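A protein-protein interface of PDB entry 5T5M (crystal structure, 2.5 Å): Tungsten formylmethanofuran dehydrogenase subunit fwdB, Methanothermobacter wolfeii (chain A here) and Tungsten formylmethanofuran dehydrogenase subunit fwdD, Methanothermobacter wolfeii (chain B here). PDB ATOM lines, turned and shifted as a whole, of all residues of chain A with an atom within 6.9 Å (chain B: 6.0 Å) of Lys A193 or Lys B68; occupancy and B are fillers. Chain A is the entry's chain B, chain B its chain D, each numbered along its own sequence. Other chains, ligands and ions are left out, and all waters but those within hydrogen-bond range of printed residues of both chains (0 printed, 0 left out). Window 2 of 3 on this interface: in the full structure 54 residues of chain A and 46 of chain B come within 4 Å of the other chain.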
ATOM      1  N   LEU A 181      -6.966  22.028  18.767  1.00  0.00           N
ATOM      2  CA  LEU A 181      -6.305  20.819  19.237  1.00  0.00           C
ATOM      3  C   LEU A 181      -5.655  20.096  18.057  1.00  0.00           C
ATOM      4  O   LEU A 181      -6.335  19.751  17.079  1.00  0.00           O
ATOM      5  CB  LEU A 181      -7.315  19.913  19.943  1.00  0.00           C
ATOM      6  CG  LEU A 181      -6.772  18.681  20.659  1.00  0.00           C
ATOM      7  CD1 LEU A 181      -5.807  19.068  21.764  1.00  0.00           C
ATOM      8  CD2 LEU A 181      -7.915  17.866  21.234  1.00  0.00           C
ATOM      9  N   VAL A 183      -3.055  16.835  17.045  1.00  0.00           N
ATOM     10  CA  VAL A 183      -2.337  15.616  17.401  1.00  0.00           C
ATOM     11  C   VAL A 183      -1.535  15.151  16.193  1.00  0.00           C
ATOM     12  O   VAL A 183      -2.065  15.085  15.078  1.00  0.00           O
ATOM     13  CB  VAL A 183      -3.294  14.509  17.870  1.00  0.00           C
ATOM     14  CG1 VAL A 183      -2.543  13.200  18.057  1.00  0.00           C
ATOM     15  CG2 VAL A 183      -3.983  14.931  19.154  1.00  0.00           C
ATOM     16  N   LYS A 188      -4.404   6.472  14.271  1.00  0.00           N
ATOM     17  CA  LYS A 188      -5.648   7.147  14.661  1.00  0.00           C
ATOM     18  C   LYS A 188      -5.940   6.810  16.125  1.00  0.00           C
ATOM     19  O   LYS A 188      -6.799   5.991  16.452  1.00  0.00           O
ATOM     20  CB  LYS A 188      -6.801   6.718  13.757  1.00  0.00           C
ATOM     21  CG  LYS A 188      -7.288   7.764  12.768  1.00  0.00           C
ATOM     22  CD  LYS A 188      -8.029   8.914  13.457  1.00  0.00           C
ATOM     23  CE  LYS A 188      -8.295  10.072  12.482  1.00  0.00           C
ATOM     24  NZ  LYS A 188      -8.785  11.317  13.150  1.00  0.00           N
ATOM     25  N   THR A 189      -5.203   7.456  17.025  1.00  0.00           N
ATOM     26  CA  THR A 189      -5.373   7.171  18.442  1.00  0.00           C
ATOM     27  C   THR A 189      -6.685   7.748  18.956  1.00  0.00           C
ATOM     28  O   THR A 189      -7.343   8.570  18.305  1.00  0.00           O
ATOM     29  CB  THR A 189      -4.245   7.770  19.275  1.00  0.00           C
ATOM     30  OG1 THR A 189      -4.241   9.192  19.108  1.00  0.00           O
ATOM     31  CG2 THR A 189      -2.891   7.179  18.888  1.00  0.00           C
ATOM     32  N   ASP A 190      -7.051   7.321  20.165  1.00  0.00           N
ATOM     33  CA  ASP A 190      -8.186   7.923  20.848  1.00  0.00           C
ATOM     34  C   ASP A 190      -7.913   9.372  21.223  1.00  0.00           C
ATOM     35  O   ASP A 190      -8.860  10.140  21.409  1.00  0.00           O
ATOM     36  CB  ASP A 190      -8.542   7.098  22.080  1.00  0.00           C
ATOM     37  CG  ASP A 190      -9.099   5.730  21.719  1.00  0.00           C
ATOM     38  OD1 ASP A 190      -9.931   5.655  20.791  1.00  0.00           O
ATOM     39  OD2 ASP A 190      -8.696   4.734  22.357  1.00  0.00           O
ATOM     40  N   SER A 191      -6.642   9.768  21.313  1.00  0.00           N
ATOM     41  CA  SER A 191      -6.319  11.179  21.474  1.00  0.00           C
ATOM     42  C   SER A 191      -6.547  11.937  20.171  1.00  0.00           C
ATOM     43  O   SER A 191      -7.183  13.000  20.159  1.00  0.00           O
ATOM     44  CB  SER A 191      -4.873  11.328  21.938  1.00  0.00           C
ATOM     45  OG  SER A 191      -4.663  10.681  23.182  1.00  0.00           O
ATOM     46  N   ALA A 192      -6.045  11.391  19.061  1.00  0.00           N
ATOM     47  CA  ALA A 192      -6.248  12.007  17.754  1.00  0.00           C
ATOM     48  C   ALA A 192      -7.725  12.112  17.396  1.00  0.00           C
ATOM     49  O   ALA A 192      -8.114  13.007  16.637  1.00  0.00           O
ATOM     50  CB  ALA A 192      -5.511  11.204  16.686  1.00  0.00           C
ATOM     51  N   LYS A 193      -8.560  11.204  17.917  1.00  0.00           N
ATOM     52  CA  LYS A 193      -9.992  11.271  17.632  1.00  0.00           C
ATOM     53  C   LYS A 193     -10.612  12.568  18.138  1.00  0.00           C
ATOM     54  O   LYS A 193     -11.567  13.072  17.540  1.00  0.00           O
ATOM     55  CB  LYS A 193     -10.707  10.073  18.247  1.00  0.00           C
ATOM     56  CG  LYS A 193     -10.503   8.790  17.465  1.00  0.00           C
ATOM     57  CD  LYS A 193     -11.029   7.551  18.202  1.00  0.00           C
ATOM     58  CE  LYS A 193     -10.597   6.275  17.467  1.00  0.00           C
ATOM     59  NZ  LYS A 193     -10.767   5.037  18.268  1.00  0.00           N
ATOM     60  N   LEU A 194     -10.082  13.128  19.219  1.00  0.00           N
ATOM     61  CA  LEU A 194     -10.606  14.368  19.773  1.00  0.00           C
ATOM     62  C   LEU A 194     -10.035  15.616  19.114  1.00  0.00           C
ATOM     63  O   LEU A 194     -10.492  16.716  19.434  1.00  0.00           O
ATOM     64  CB  LEU A 194     -10.322  14.416  21.277  1.00  0.00           C
ATOM     65  CG  LEU A 194     -10.887  13.250  22.085  1.00  0.00           C
ATOM     66  CD1 LEU A 194     -10.485  13.403  23.526  1.00  0.00           C
ATOM     67  CD2 LEU A 194     -12.399  13.195  21.957  1.00  0.00           C
ATOM     68  N   ALA A 195      -9.079  15.481  18.199  1.00  0.00           N
ATOM     69  CA  ALA A 195      -8.347  16.635  17.702  1.00  0.00           C
ATOM     70  C   ALA A 195      -9.128  17.378  16.621  1.00  0.00           C
ATOM     71  O   ALA A 195     -10.002  16.831  15.952  1.00  0.00           O
ATOM     72  CB  ALA A 195      -6.988  16.205  17.144  1.00  0.00           C
ATOM     73  N   ASP A 196      -8.792  18.654  16.463  1.00  0.00           N
ATOM     74  CA  ASP A 196      -9.270  19.436  15.329  1.00  0.00           C
ATOM     75  C   ASP A 196      -8.424  19.201  14.086  1.00  0.00           C
ATOM     76  O   ASP A 196      -8.932  19.296  12.966  1.00  0.00           O
ATOM     77  CB  ASP A 196      -9.256  20.924  15.684  1.00  0.00           C
ATOM     78  CG  ASP A 196     -10.211  21.254  16.794  1.00  0.00           C
ATOM     79  OD1 ASP A 196     -11.378  20.819  16.686  1.00  0.00           O
ATOM     80  OD2 ASP A 196      -9.792  21.918  17.775  1.00  0.00           O
ATOM     81  N   HIS A 198      -5.466  16.327  12.818  1.00  0.00           N
ATOM     82  CA  HIS A 198      -4.653  15.138  13.037  1.00  0.00           C
ATOM     83  C   HIS A 198      -3.657  15.054  11.892  1.00  0.00           C
ATOM     84  O   HIS A 198      -4.052  14.841  10.741  1.00  0.00           O
ATOM     85  CB  HIS A 198      -5.508  13.877  13.090  1.00  0.00           C
ATOM     86  CG  HIS A 198      -4.716  12.617  13.245  1.00  0.00           C
ATOM     87  ND1 HIS A 198      -5.212  11.380  12.895  1.00  0.00           N
ATOM     88  CD2 HIS A 198      -3.470  12.398  13.729  1.00  0.00           C
ATOM     89  CE1 HIS A 198      -4.303  10.454  13.152  1.00  0.00           C
ATOM     90  NE2 HIS A 198      -3.239  11.045  13.663  1.00  0.00           N
ATOM     91  N   TRP B  12      -5.463  -0.308  29.064  1.00  0.00           N
ATOM     92  CA  TRP B  12      -5.635  -1.631  29.661  1.00  0.00           C
ATOM     93  C   TRP B  12      -4.313  -2.184  30.170  1.00  0.00           C
ATOM     94  O   TRP B  12      -4.269  -2.841  31.217  1.00  0.00           O
ATOM     95  CB  TRP B  12      -6.257  -2.593  28.653  1.00  0.00           C
ATOM     96  CG  TRP B  12      -7.409  -1.981  27.975  1.00  0.00           C
ATOM     97  CD1 TRP B  12      -7.526  -1.719  26.653  1.00  0.00           C
ATOM     98  CD2 TRP B  12      -8.610  -1.505  28.593  1.00  0.00           C
ATOM     99  NE1 TRP B  12      -8.734  -1.120  26.395  1.00  0.00           N
ATOM    100  CE2 TRP B  12      -9.420  -0.975  27.572  1.00  0.00           C
ATOM    101  CE3 TRP B  12      -9.081  -1.480  29.909  1.00  0.00           C
ATOM    102  CZ2 TRP B  12     -10.676  -0.429  27.822  1.00  0.00           C
ATOM    103  CZ3 TRP B  12     -10.325  -0.940  30.157  1.00  0.00           C
ATOM    104  CH2 TRP B  12     -11.112  -0.420  29.117  1.00  0.00           C
ATOM    105  N   GLN B  34      -1.987  -5.823  18.104  1.00  0.00           N
ATOM    106  CA  GLN B  34      -3.108  -5.144  17.465  1.00  0.00           C
ATOM    107  C   GLN B  34      -2.859  -5.029  15.968  1.00  0.00           C
ATOM    108  O   GLN B  34      -1.784  -4.602  15.542  1.00  0.00           O
ATOM    109  CB  GLN B  34      -3.301  -3.753  18.069  1.00  0.00           C
ATOM    110  CG  GLN B  34      -3.580  -3.752  19.556  1.00  0.00           C
ATOM    111  CD  GLN B  34      -3.788  -2.364  20.111  1.00  0.00           C
ATOM    112  OE1 GLN B  34      -3.854  -1.382  19.369  1.00  0.00           O
ATOM    113  NE2 GLN B  34      -3.895  -2.272  21.429  1.00  0.00           N
ATOM    114  N   GLU B  66      -7.983  -7.215  17.014  1.00  0.00           N
ATOM    115  CA  GLU B  66      -8.344  -6.107  16.147  1.00  0.00           C
ATOM    116  C   GLU B  66      -8.062  -4.787  16.855  1.00  0.00           C
ATOM    117  O   GLU B  66      -8.400  -4.609  18.030  1.00  0.00           O
ATOM    118  CB  GLU B  66      -9.811  -6.205  15.740  1.00  0.00           C
ATOM    119  CG  GLU B  66     -10.198  -5.247  14.630  1.00  0.00           C
ATOM    120  CD  GLU B  66     -11.559  -5.554  14.026  1.00  0.00           C
ATOM    121  OE1 GLU B  66     -11.968  -6.738  14.020  1.00  0.00           O
ATOM    122  OE2 GLU B  66     -12.224  -4.609  13.554  1.00  0.00           O
ATOM    123  N   ALA B  67      -7.425  -3.867  16.141  1.00  0.00           N
ATOM    124  CA  ALA B  67      -7.039  -2.589  16.715  1.00  0.00           C
ATOM    125  C   ALA B  67      -8.243  -1.658  16.734  1.00  0.00           C
ATOM    126  O   ALA B  67      -8.790  -1.321  15.676  1.00  0.00           O
ATOM    127  CB  ALA B  67      -5.902  -1.968  15.912  1.00  0.00           C
ATOM    128  N   LYS B  68      -8.663  -1.252  17.938  1.00  0.00           N
ATOM    129  CA  LYS B  68      -9.665  -0.199  18.058  1.00  0.00           C
ATOM    130  C   LYS B  68      -9.084   1.177  17.743  1.00  0.00           C
ATOM    131  O   LYS B  68      -9.849   2.107  17.479  1.00  0.00           O
ATOM    132  CB  LYS B  68     -10.274  -0.181  19.462  1.00  0.00           C
ATOM    133  CG  LYS B  68     -11.066  -1.416  19.868  1.00  0.00           C
ATOM    134  CD  LYS B  68     -11.562  -1.253  21.313  1.00  0.00           C
ATOM    135  CE  LYS B  68     -12.391  -2.427  21.822  1.00  0.00           C
ATOM    136  NZ  LYS B  68     -12.826  -2.211  23.247  1.00  0.00           N
ATOM    137  N   GLU B  69      -7.756   1.331  17.787  1.00  0.00           N
ATOM    138  CA  GLU B  69      -7.099   2.559  17.348  1.00  0.00           C
ATOM    139  C   GLU B  69      -6.446   2.305  15.992  1.00  0.00           C
ATOM    140  O   GLU B  69      -5.323   1.782  15.940  1.00  0.00           O
ATOM    141  CB  GLU B  69      -6.060   3.023  18.370  1.00  0.00           C
ATOM    142  CG  GLU B  69      -6.684   3.617  19.625  1.00  0.00           C
ATOM    143  CD  GLU B  69      -5.662   3.952  20.700  1.00  0.00           C
ATOM    144  OE1 GLU B  69      -5.553   5.142  21.069  1.00  0.00           O
ATOM    145  OE2 GLU B  69      -4.967   3.028  21.176  1.00  0.00           O
ATOM    146  N   PRO B  70      -7.095   2.659  14.882  1.00  0.00           N
ATOM    147  CA  PRO B  70      -6.628   2.202  13.564  1.00  0.00           C
ATOM    148  C   PRO B  70      -5.174   2.555  13.292  1.00  0.00           C
ATOM    149  O   PRO B  70      -4.686   3.622  13.672  1.00  0.00           O
ATOM    150  CB  PRO B  70      -7.566   2.920  12.591  1.00  0.00           C
ATOM    151  CG  PRO B  70      -8.829   3.133  13.386  1.00  0.00           C
ATOM    152  CD  PRO B  70      -8.369   3.394  14.796  1.00  0.00           C
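The backbone NH (N) of Ser A191 lies close to the side-chain hydroxyl (OG1) of Thr A189, at 3.3 Å.
N of Ala A192 is in hydrogen-bond range of OG1 of Thr A189 (2.8 Å).
The side-chain carboxylate (OD1) of Asp A190 is in salt-bridge range of the side-chain amino group (NZ) of Lys A193.
N of Lys A188 lies within hydrogen-bond range of O of Pro B70 (2.9 Å).
The side-chain carboxylate (OE1) of Glu B69 lies within hydrogen-bond range of the backbone NH (N) of Asp A190 (2.8 Å).
NZ of Lys A193 is in hydrogen-bond range of O of Lys B68 (3.2 Å).
Among the printed residues, merely in contact across the chains: Lys A188 with Glu B69 and Thr A189 with Glu B69.
Of chain B, only Lys B68 comes within 4 Å of Lys A193.
Of chain A, only Lys A193 (3.2 Å) comes within 4 Å of Lys B68.
Of the printed residues of chain A, Pro B70 touches Lys A188 (2.9 Å).
Printed residues of chain B within 4 Å of Lys A188: Glu B69 (3.6 Å) and Pro B70 (2.9 Å).
Of the printed residues of chain B, Asp A190 touches Glu B69 (2.8 Å).
Of the printed residues of chain A, Glu B69 touches Lys A188, Thr A189 and Asp A190.
Of the printed residues of chain B, Thr A189 touches Glu B69.
Trp B12 touches none of the printed residues of chain A.
The nearest printed residue of chain B that does not touch Lys A193 is Pro B70 (4.5 Å).
The nearest residue of chain A that does not touch Lys B68 is Asp A190 (4.9 Å).
Printed residues of chain A that touch a printed residue of chain B: Lys A188, Thr A189, Asp A190 and Lys A193.
Of the 7 printed residues of chain B, 3 touch a printed residue of chain A.
Hydrophobic or aromatic side chains of chain B that line the printed part of chain A: Pro B70.
Among the printed residues, 5 pairs touch across the chains.
Among the printed residues, no Asp or Glu carboxylate lies within 4 Å of a Lys or Arg side-chain nitrogen of the other chain.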
